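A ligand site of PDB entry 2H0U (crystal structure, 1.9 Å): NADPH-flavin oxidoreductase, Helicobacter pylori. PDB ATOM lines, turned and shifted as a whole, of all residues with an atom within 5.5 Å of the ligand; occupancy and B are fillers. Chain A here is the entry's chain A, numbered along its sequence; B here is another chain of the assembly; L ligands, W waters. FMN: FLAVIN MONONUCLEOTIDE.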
ATOM      1  N   ARG A  13       4.751  -3.699   5.167  1.00  0.00           N
ATOM      2  CA  ARG A  13       4.609  -2.841   6.338  1.00  0.00           C
ATOM      3  C   ARG A  13       3.269  -2.101   6.149  1.00  0.00           C
ATOM      4  O   ARG A  13       3.138  -1.316   5.227  1.00  0.00           O
ATOM      5  CB  ARG A  13       5.777  -1.821   6.386  1.00  0.00           C
ATOM      6  CG  ARG A  13       6.104  -1.214   7.800  1.00  0.00           C
ATOM      7  CD  ARG A  13       5.065  -0.164   8.314  1.00  0.00           C
ATOM      8  NE  ARG A  13       4.598   0.687   7.205  1.00  0.00           N
ATOM      9  CZ  ARG A  13       3.399   1.252   7.128  1.00  0.00           C
ATOM     10  NH1 ARG A  13       2.532   1.129   8.126  1.00  0.00           N
ATOM     11  NH2 ARG A  13       3.067   1.918   6.024  1.00  0.00           N
ATOM     12  N   PHE A  14       2.287  -2.374   7.002  1.00  0.00           N
ATOM     13  CA  PHE A  14       1.026  -1.658   6.927  1.00  0.00           C
ATOM     14  C   PHE A  14       0.542  -1.465   8.355  1.00  0.00           C
ATOM     15  O   PHE A  14       1.101  -2.036   9.287  1.00  0.00           O
ATOM     16  CB  PHE A  14      -0.021  -2.425   6.106  1.00  0.00           C
ATOM     17  CG  PHE A  14      -0.650  -3.584   6.844  1.00  0.00           C
ATOM     18  CD1 PHE A  14      -1.973  -3.506   7.318  1.00  0.00           C
ATOM     19  CD2 PHE A  14       0.087  -4.775   7.045  1.00  0.00           C
ATOM     20  CE1 PHE A  14      -2.542  -4.610   7.986  1.00  0.00           C
ATOM     21  CE2 PHE A  14      -0.472  -5.845   7.751  1.00  0.00           C
ATOM     22  CZ  PHE A  14      -1.772  -5.775   8.210  1.00  0.00           C
ATOM     23  N   ALA A  15      -0.488  -0.658   8.521  1.00  0.00           N
ATOM     24  CA  ALA A  15      -0.986  -0.397   9.867  1.00  0.00           C
ATOM     25  C   ALA A  15      -1.900  -1.550  10.289  1.00  0.00           C
ATOM     26  O   ALA A  15      -3.123  -1.587   9.986  1.00  0.00           O
ATOM     27  CB  ALA A  15      -1.708   0.971   9.925  1.00  0.00           C
ATOM     28  N   LYS A  17      -4.240  -3.625  12.408  1.00  0.00           N
ATOM     29  CA  LYS A  17      -5.223  -3.331  13.468  1.00  0.00           C
ATOM     30  C   LYS A  17      -5.721  -4.568  14.205  1.00  0.00           C
ATOM     31  O   LYS A  17      -6.318  -4.445  15.292  1.00  0.00           O
ATOM     32  CB  LYS A  17      -6.453  -2.593  12.917  1.00  0.00           C
ATOM     33  CG  LYS A  17      -6.251  -1.198  12.253  1.00  0.00           C
ATOM     34  CD  LYS A  17      -4.961  -0.464  12.612  1.00  0.00           C
ATOM     35  CE  LYS A  17      -4.758   0.727  11.660  1.00  0.00           C
ATOM     36  NZ  LYS A  17      -6.018   1.538  11.381  1.00  0.00           N
ATOM     37  N   TYR A 143      10.109  10.199  15.932  1.00  0.00           N
ATOM     38  CA  TYR A 143       9.356   9.573  14.816  1.00  0.00           C
ATOM     39  C   TYR A 143      10.320   8.763  13.951  1.00  0.00           C
ATOM     40  O   TYR A 143       9.926   7.760  13.386  1.00  0.00           O
ATOM     41  CB  TYR A 143       8.575  10.614  13.998  1.00  0.00           C
ATOM     42  CG  TYR A 143       7.188  10.938  14.593  1.00  0.00           C
ATOM     43  CD1 TYR A 143       7.080  11.420  15.903  1.00  0.00           C
ATOM     44  CD2 TYR A 143       6.004  10.731  13.859  1.00  0.00           C
ATOM     45  CE1 TYR A 143       5.812  11.716  16.504  1.00  0.00           C
ATOM     46  CE2 TYR A 143       4.729  11.053  14.422  1.00  0.00           C
ATOM     47  CZ  TYR A 143       4.673  11.530  15.759  1.00  0.00           C
ATOM     48  OH  TYR A 143       3.493  11.832  16.368  1.00  0.00           O
ATOM     49  N   MET A 146      10.846   5.536  15.916  1.00  0.00           N
ATOM     50  CA  MET A 146       9.682   4.632  15.751  1.00  0.00           C
ATOM     51  C   MET A 146       9.604   4.062  14.329  1.00  0.00           C
ATOM     52  O   MET A 146       9.357   2.854  14.150  1.00  0.00           O
ATOM     53  CB  MET A 146       8.376   5.398  16.107  1.00  0.00           C
ATOM     54  CG  MET A 146       7.139   4.607  15.738  1.00  0.00           C
ATOM     55  SD  MET A 146       5.470   5.607  15.951  1.00  0.00           S
ATOM     56  CE  MET A 146       5.660   6.861  14.452  1.00  0.00           C
ATOM     57  N   CYS A 161       1.683  -0.999  14.301  1.00  0.00           N
ATOM     58  CA  CYS A 161       0.813   0.121  14.019  1.00  0.00           C
ATOM     59  C   CYS A 161       1.301   1.325  14.802  1.00  0.00           C
ATOM     60  O   CYS A 161       1.484   1.244  16.029  1.00  0.00           O
ATOM     61  CB  CYS A 161      -0.661  -0.201  14.356  1.00  0.00           C
ATOM     62  SG  CYS A 161      -1.802   1.131  13.751  1.00  0.00           S
ATOM     63  N   PRO A 162       1.550   2.456  14.094  1.00  0.00           N
ATOM     64  CA  PRO A 162       1.904   3.718  14.769  1.00  0.00           C
ATOM     65  C   PRO A 162       0.618   4.238  15.399  1.00  0.00           C
ATOM     66  O   PRO A 162      -0.460   4.026  14.837  1.00  0.00           O
ATOM     67  CB  PRO A 162       2.292   4.651  13.621  1.00  0.00           C
ATOM     68  CG  PRO A 162       2.183   3.848  12.352  1.00  0.00           C
ATOM     69  CD  PRO A 162       1.394   2.630  12.636  1.00  0.00           C
ATOM     70  N   ILE A 163       0.741   4.926  16.525  1.00  0.00           N
ATOM     71  CA  ILE A 163      -0.440   5.299  17.306  1.00  0.00           C
ATOM     72  C   ILE A 163      -0.280   6.724  17.875  1.00  0.00           C
ATOM     73  O   ILE A 163       0.588   6.968  18.700  1.00  0.00           O
ATOM     74  CB  ILE A 163      -0.735   4.287  18.475  1.00  0.00           C
ATOM     75  CG1 ILE A 163      -1.052   2.863  17.977  1.00  0.00           C
ATOM     76  CG2 ILE A 163      -1.887   4.826  19.398  1.00  0.00           C
ATOM     77  CD1 ILE A 163      -1.000   1.802  19.105  1.00  0.00           C
ATOM     78  N   GLU A 164      -1.144   7.636  17.420  1.00  0.00           N
ATOM     79  CA  GLU A 164      -1.272   8.963  17.994  1.00  0.00           C
ATOM     80  C   GLU A 164      -2.613   9.139  18.717  1.00  0.00           C
ATOM     81  O   GLU A 164      -2.785  10.126  19.414  1.00  0.00           O
ATOM     82  CB  GLU A 164      -1.167  10.050  16.886  1.00  0.00           C
ATOM     83  CG  GLU A 164       0.271  10.359  16.424  1.00  0.00           C
ATOM     84  CD  GLU A 164       0.298  11.415  15.295  1.00  0.00           C
ATOM     85  OE1 GLU A 164      -0.784  11.929  14.946  1.00  0.00           O
ATOM     86  OE2 GLU A 164       1.399  11.757  14.817  1.00  0.00           O
ATOM     87  N   GLY A 165      -3.522   8.194  18.544  1.00  0.00           N
ATOM     88  CA  GLY A 165      -4.927   8.302  19.038  1.00  0.00           C
ATOM     89  C   GLY A 165      -5.120   8.035  20.540  1.00  0.00           C
ATOM     90  O   GLY A 165      -5.683   7.018  20.951  1.00  0.00           O
ATOM     91  N   VAL A 190       4.700   9.776  21.003  1.00  0.00           N
ATOM     92  CA  VAL A 190       3.890   8.949  20.074  1.00  0.00           C
ATOM     93  C   VAL A 190       3.918   7.533  20.644  1.00  0.00           C
ATOM     94  O   VAL A 190       4.672   7.281  21.620  1.00  0.00           O
ATOM     95  CB  VAL A 190       4.438   9.048  18.618  1.00  0.00           C
ATOM     96  CG1 VAL A 190       5.884   8.459  18.495  1.00  0.00           C
ATOM     97  CG2 VAL A 190       3.433   8.483  17.572  1.00  0.00           C
ATOM     98  N   THR A 202      -3.473  -4.681   4.375  1.00  0.00           N
ATOM     99  CA  THR A 202      -4.362  -3.652   3.797  1.00  0.00           C
ATOM    100  C   THR A 202      -3.649  -3.054   2.577  1.00  0.00           C
ATOM    101  O   THR A 202      -2.542  -2.542   2.742  1.00  0.00           O
ATOM    102  CB  THR A 202      -4.589  -2.534   4.843  1.00  0.00           C
ATOM    103  OG1 THR A 202      -5.097  -3.131   6.049  1.00  0.00           O
ATOM    104  CG2 THR A 202      -5.610  -1.451   4.345  1.00  0.00           C
ATOM    105  N   LYS A 204      -2.241  -0.505  -0.133  1.00  0.00           N
ATOM    106  CA  LYS A 204      -1.876   0.902   0.012  1.00  0.00           C
ATOM    107  C   LYS A 204      -2.798   1.776  -0.810  1.00  0.00           C
ATOM    108  O   LYS A 204      -3.137   1.422  -1.953  1.00  0.00           O
ATOM    109  CB  LYS A 204      -0.431   1.110  -0.454  1.00  0.00           C
ATOM    110  CG  LYS A 204       0.573   0.543   0.475  1.00  0.00           C
ATOM    111  CD  LYS A 204       0.909   1.560   1.589  1.00  0.00           C
ATOM    112  CE  LYS A 204       1.946   0.994   2.594  1.00  0.00           C
ATOM    113  NZ  LYS A 204       1.312  -0.033   3.546  1.00  0.00           N
ATOM    114  N   ARG A 206      -2.398   5.800  -1.791  1.00  0.00           N
ATOM    115  CA  ARG A 206      -1.529   6.987  -1.667  1.00  0.00           C
ATOM    116  C   ARG A 206      -1.769   7.914  -2.835  1.00  0.00           C
ATOM    117  O   ARG A 206      -2.242   7.472  -3.895  1.00  0.00           O
ATOM    118  CB  ARG A 206      -0.033   6.564  -1.685  1.00  0.00           C
ATOM    119  CG  ARG A 206       0.483   5.797  -0.442  1.00  0.00           C
ATOM    120  CD  ARG A 206       0.367   6.628   0.861  1.00  0.00           C
ATOM    121  NE  ARG A 206       0.995   5.914   1.979  1.00  0.00           N
ATOM    122  CZ  ARG A 206       0.404   4.960   2.684  1.00  0.00           C
ATOM    123  NH1 ARG A 206      -0.851   4.609   2.456  1.00  0.00           N
ATOM    124  NH2 ARG A 206       1.084   4.352   3.642  1.00  0.00           N
ATOM    125  N   LEU B  39       5.058   5.764  -0.276  1.00  0.00           N
ATOM    126  CA  LEU B  39       4.324   4.726   0.470  1.00  0.00           C
ATOM    127  C   LEU B  39       4.418   4.859   1.968  1.00  0.00           C
ATOM    128  O   LEU B  39       3.813   4.053   2.693  1.00  0.00           O
ATOM    129  CB  LEU B  39       4.833   3.332   0.046  1.00  0.00           C
ATOM    130  CG  LEU B  39       4.581   3.054  -1.440  1.00  0.00           C
ATOM    131  CD1 LEU B  39       5.276   1.763  -1.760  1.00  0.00           C
ATOM    132  CD2 LEU B  39       3.061   2.928  -1.741  1.00  0.00           C
ATOM    133  N   ALA B  40       5.147   5.861   2.476  1.00  0.00           N
ATOM    134  CA  ALA B  40       5.220   6.033   3.924  1.00  0.00           C
ATOM    135  C   ALA B  40       3.861   6.240   4.593  1.00  0.00           C
ATOM    136  O   ALA B  40       2.957   6.854   3.996  1.00  0.00           O
ATOM    137  CB  ALA B  40       6.155   7.212   4.292  1.00  0.00           C
ATOM    138  N   PRO B  41       3.700   5.741   5.841  1.00  0.00           N
ATOM    139  CA  PRO B  41       2.441   6.000   6.606  1.00  0.00           C
ATOM    140  C   PRO B  41       2.429   7.375   7.194  1.00  0.00           C
ATOM    141  O   PRO B  41       3.509   8.001   7.390  1.00  0.00           O
ATOM    142  CB  PRO B  41       2.486   4.970   7.734  1.00  0.00           C
ATOM    143  CG  PRO B  41       4.053   4.727   7.966  1.00  0.00           C
ATOM    144  CD  PRO B  41       4.680   4.916   6.580  1.00  0.00           C
ATOM    145  N   SER B  42       1.230   7.856   7.501  1.00  0.00           N
ATOM    146  CA  SER B  42       1.080   9.166   8.143  1.00  0.00           C
ATOM    147  C   SER B  42      -0.158   9.106   9.009  1.00  0.00           C
ATOM    148  O   SER B  42      -1.065   8.321   8.742  1.00  0.00           O
ATOM    149  CB  SER B  42       0.918  10.273   7.103  1.00  0.00           C
ATOM    150  OG  SER B  42      -0.126   9.938   6.183  1.00  0.00           O
ATOM    151  N   SER B  43      -0.212   9.967  10.021  1.00  0.00           N
ATOM    152  CA  SER B  43      -1.386  10.033  10.891  1.00  0.00           C
ATOM    153  C   SER B  43      -2.650  10.324  10.073  1.00  0.00           C
ATOM    154  O   SER B  43      -2.673  11.270   9.268  1.00  0.00           O
ATOM    155  CB  SER B  43      -1.169  11.103  11.946  1.00  0.00           C
ATOM    156  OG  SER B  43      -2.221  11.026  12.899  1.00  0.00           O
ATOM    157  N   ILE B  44      -3.672   9.465  10.250  1.00  0.00           N
ATOM    158  CA  ILE B  44      -4.996   9.562   9.600  1.00  0.00           C
ATOM    159  C   ILE B  44      -4.853   9.336   8.093  1.00  0.00           C
ATOM    160  O   ILE B  44      -5.757   9.638   7.314  1.00  0.00           O
ATOM    161  CB  ILE B  44      -5.747  10.912   9.873  1.00  0.00           C
ATOM    162  CG1 ILE B  44      -5.400  11.490  11.267  1.00  0.00           C
ATOM    163  CG2 ILE B  44      -7.310  10.717   9.688  1.00  0.00           C
ATOM    164  CD1 ILE B  44      -6.066  12.852  11.635  1.00  0.00           C
ATOM    165  N   GLY B  45      -3.736   8.737   7.700  1.00  0.00           N
ATOM    166  CA  GLY B  45      -3.370   8.630   6.291  1.00  0.00           C
ATOM    167  C   GLY B  45      -3.396   9.895   5.423  1.00  0.00           C
ATOM    168  O   GLY B  45      -3.654   9.807   4.224  1.00  0.00           O
ATOM    169  N   LYS B 104      -8.630   8.296  -0.497  1.00  0.00           N
ATOM    170  CA  LYS B 104      -9.310   7.319   0.363  1.00  0.00           C
ATOM    171  C   LYS B 104     -10.693   6.931  -0.166  1.00  0.00           C
ATOM    172  O   LYS B 104     -11.267   5.918   0.253  1.00  0.00           O
ATOM    173  CB  LYS B 104      -9.387   7.823   1.825  1.00  0.00           C
ATOM    174  CG  LYS B 104      -8.011   8.203   2.464  1.00  0.00           C
ATOM    175  CD  LYS B 104      -6.983   7.073   2.317  1.00  0.00           C
ATOM    176  CE  LYS B 104      -5.578   7.484   2.814  1.00  0.00           C
ATOM    177  NZ  LYS B 104      -4.608   6.345   2.664  1.00  0.00           N
ATOM    178  N   GLN B 141       5.258  13.695  10.475  1.00  0.00           N
ATOM    179  CA  GLN B 141       4.918  12.638   9.520  1.00  0.00           C
ATOM    180  C   GLN B 141       6.032  12.567   8.459  1.00  0.00           C
ATOM    181  O   GLN B 141       6.418  11.466   8.059  1.00  0.00           O
ATOM    182  CB  GLN B 141       3.556  12.909   8.816  1.00  0.00           C
ATOM    183  CG  GLN B 141       2.389  13.362   9.787  1.00  0.00           C
ATOM    184  CD  GLN B 141       2.199  12.439  10.973  1.00  0.00           C
ATOM    185  OE1 GLN B 141       2.078  11.223  10.813  1.00  0.00           O
ATOM    186  NE2 GLN B 141       2.160  13.011  12.168  1.00  0.00           N
ATOM    187  N   ILE B 144       9.000  10.362   9.334  1.00  0.00           N
ATOM    188  CA  ILE B 144       8.771   8.926   8.982  1.00  0.00           C
ATOM    189  C   ILE B 144       9.139   8.715   7.499  1.00  0.00           C
ATOM    190  O   ILE B 144       9.849   7.781   7.149  1.00  0.00           O
ATOM    191  CB  ILE B 144       7.311   8.480   9.222  1.00  0.00           C
ATOM    192  CG1 ILE B 144       6.940   8.715  10.676  1.00  0.00           C
ATOM    193  CG2 ILE B 144       7.113   6.967   8.786  1.00  0.00           C
ATOM    194  CD1 ILE B 144       5.370   8.406  10.931  1.00  0.00           C
HETATM  195  N1  FMN L   1      -4.086   4.064  13.263  1.00  0.00           N
HETATM  196  C2  FMN L   1      -5.010   3.856  14.274  1.00  0.00           C
HETATM  197  O2  FMN L   1      -5.907   3.042  14.102  1.00  0.00           O
HETATM  198  N3  FMN L   1      -4.970   4.574  15.445  1.00  0.00           N
HETATM  199  C4  FMN L   1      -3.996   5.532  15.618  1.00  0.00           C
HETATM  200  O4  FMN L   1      -3.871   6.070  16.719  1.00  0.00           O
HETATM  201  C4A FMN L   1      -3.079   5.766  14.570  1.00  0.00           C
HETATM  202  N5  FMN L   1      -2.103   6.725  14.718  1.00  0.00           N
HETATM  203  C5A FMN L   1      -1.130   6.907  13.754  1.00  0.00           C
HETATM  204  C6  FMN L   1      -0.146   7.883  13.997  1.00  0.00           C
HETATM  205  C7  FMN L   1       0.841   8.067  13.013  1.00  0.00           C
HETATM  206  C7M FMN L   1       2.083   8.810  13.415  1.00  0.00           C
HETATM  207  C8  FMN L   1       0.833   7.347  11.798  1.00  0.00           C
HETATM  208  C8M FMN L   1       2.069   7.363  10.900  1.00  0.00           C
HETATM  209  C9  FMN L   1      -0.150   6.392  11.584  1.00  0.00           C
HETATM  210  C9A FMN L   1      -1.152   6.183  12.559  1.00  0.00           C
HETATM  211  N10 FMN L   1      -2.174   5.243  12.360  1.00  0.00           N
HETATM  212  C10 FMN L   1      -3.112   5.016  13.399  1.00  0.00           C
HETATM  213  C1' FMN L   1      -2.278   4.423  11.107  1.00  0.00           C
HETATM  214  C2' FMN L   1      -2.587   5.287   9.870  1.00  0.00           C
HETATM  215  O2' FMN L   1      -3.987   5.362   9.736  1.00  0.00           O
HETATM  216  C3' FMN L   1      -1.961   4.569   8.659  1.00  0.00           C
HETATM  217  O3' FMN L   1      -0.558   4.523   8.810  1.00  0.00           O
HETATM  218  C4' FMN L   1      -2.218   5.222   7.317  1.00  0.00           C
HETATM  219  O4' FMN L   1      -3.605   5.145   7.043  1.00  0.00           O
HETATM  220  C5' FMN L   1      -1.426   4.609   6.139  1.00  0.00           C
HETATM  221  O5' FMN L   1      -1.803   3.228   6.055  1.00  0.00           O
HETATM  222  P   FMN L   1      -0.685   2.089   6.173  1.00  0.00           P
HETATM  223  O1P FMN L   1       0.068   2.364   7.443  1.00  0.00           O
HETATM  224  O2P FMN L   1      -1.444   0.760   6.246  1.00  0.00           O
HETATM  225  O3P FMN L   1       0.228   2.125   4.972  1.00  0.00           O
HETATM  226  O   HOH W   1      -1.899   0.085   3.668  1.00  0.00           O
HETATM  227  O   HOH W   2      -5.621   3.487  18.198  1.00  0.00           O
HETATM  228  O   HOH W   3      -5.158   2.798   8.902  1.00  0.00           O
HETATM  229  O   HOH W   4      -7.127   6.337   9.773  1.00  0.00           O
HETATM  230  O   HOH W   5      -4.578   7.346  11.885  1.00  0.00           O
HETATM  231  O   HOH W   6      -4.275   1.283   6.929  1.00  0.00           O
HETATM  232  O   HOH W   7      -4.362   8.934  13.957  1.00  0.00           O
HETATM  233  O   HOH W   8      -2.899   2.613   2.804  1.00  0.00           O
HETATM  234  O   HOH W   9      -4.574   4.271   4.558  1.00  0.00           O
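NE2 of Gln 141 of chain B sits at hydrogen-bond distance from OE2 of Glu 164, 3.0 Å away.
The side-chain carboxylate (OE2) of Glu 164 is in hydrogen-bond range of the side-chain hydroxyl (OH) of Tyr 143.
The side-chain carboxylate of Glu 164 sits at hydrogen-bond distance from the side-chain hydroxyl of Ser 43 of chain B.
N of Ser 43 of chain B is in hydrogen-bond range of OE1 of Gln 141 of chain B (2.7 Å).
NH2 of Arg 206 lies within hydrogen-bond range of O of Leu 39 of chain B.
The backbone carbonyl oxygen (O) of Ala 40 of chain B lies within hydrogen-bond range of the guanidinium group (NE) of Arg 206.
The side-chain amino group (NZ) of Lys 204 sits at hydrogen-bond distance from the backbone carbonyl oxygen (O) of Arg 13 (2.8 Å).
Water W1 lies within hydrogen-bond range of O2P of the ligand, O of Thr 202 and NZ of Lys 204.
Water W9 lies within hydrogen-bond range of an oxygen (O4') of the ligand (2.8 Å) and the side-chain amino group of Lys 104 of chain B (2.8 Å).
Water W3 bridges the side-chain amino group (NZ) of Lys 17 (2.9 Å) and an oxygen (O2') of the ligand (2.9 Å).
Water W5 lies within hydrogen-bond range of N of Ile 44 of chain B and O2' of the ligand.
Water W7 bridges the side-chain hydroxyl (OG) of Ser 43 of chain B and a nitrogen (N5) of the ligand.
Water W8 lies within hydrogen-bond range of NH1 of Arg 206 (2.9 Å) and O5' of the ligand (3.5 Å).
The guanidinium group (NH1) of Arg 13 is in salt-bridge range of an oxygen (O1P) of the ligand, at 2.8 Å.
The backbone NH (N) of Ala 15 is in hydrogen-bond range of an oxygen (O2P) of the ligand.
An oxygen (O4) of the ligand is in hydrogen-bond range of the backbone NH of Gly 165.
The side-chain amino group (NZ) of Lys 17 is in hydrogen-bond range of an oxygen (O2) of the ligand (3.1 Å).
The backbone NH (N) of Glu 164 lies within hydrogen-bond range of a nitrogen (N5) of the ligand (3.0 Å).
The side-chain amino group (NZ) of Lys 204 is in salt-bridge range of an oxygen (O3P) of the ligand (2.8 Å).
O3P of the ligand is in salt-bridge range of NH2 of Arg 206, at 2.7 Å.
The side-chain sulfur (SG) of Cys 161 sits at hydrogen-bond distance from a nitrogen (N1) of the ligand (3.7 Å).
N5 of the ligand lies close to O of Pro 162, at 3.2 Å.
Phe 14 touches the ligand.
Tyr 143 touches the ligand.
CA of Ile 163 touches N5 of the ligand, 3.4 Å away.
CB of Pro 41 of chain B touches O3' of the ligand, at 3.3 Å.
Ser 42 of chain B touches the ligand.
Ser 43 of chain B touches the ligand (N to C8, 3.3 Å).
Gly 45 of chain B touches the ligand.
OE1 of Gln 141 of chain B touches C7M of the ligand, 3.5 Å away.
CD1 of Ile 144 of chain B touches C8M of the ligand (3.5 Å).
The nearest printed residue that does not touch the ligand is Ile 44 of chain B (4.1 Å).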
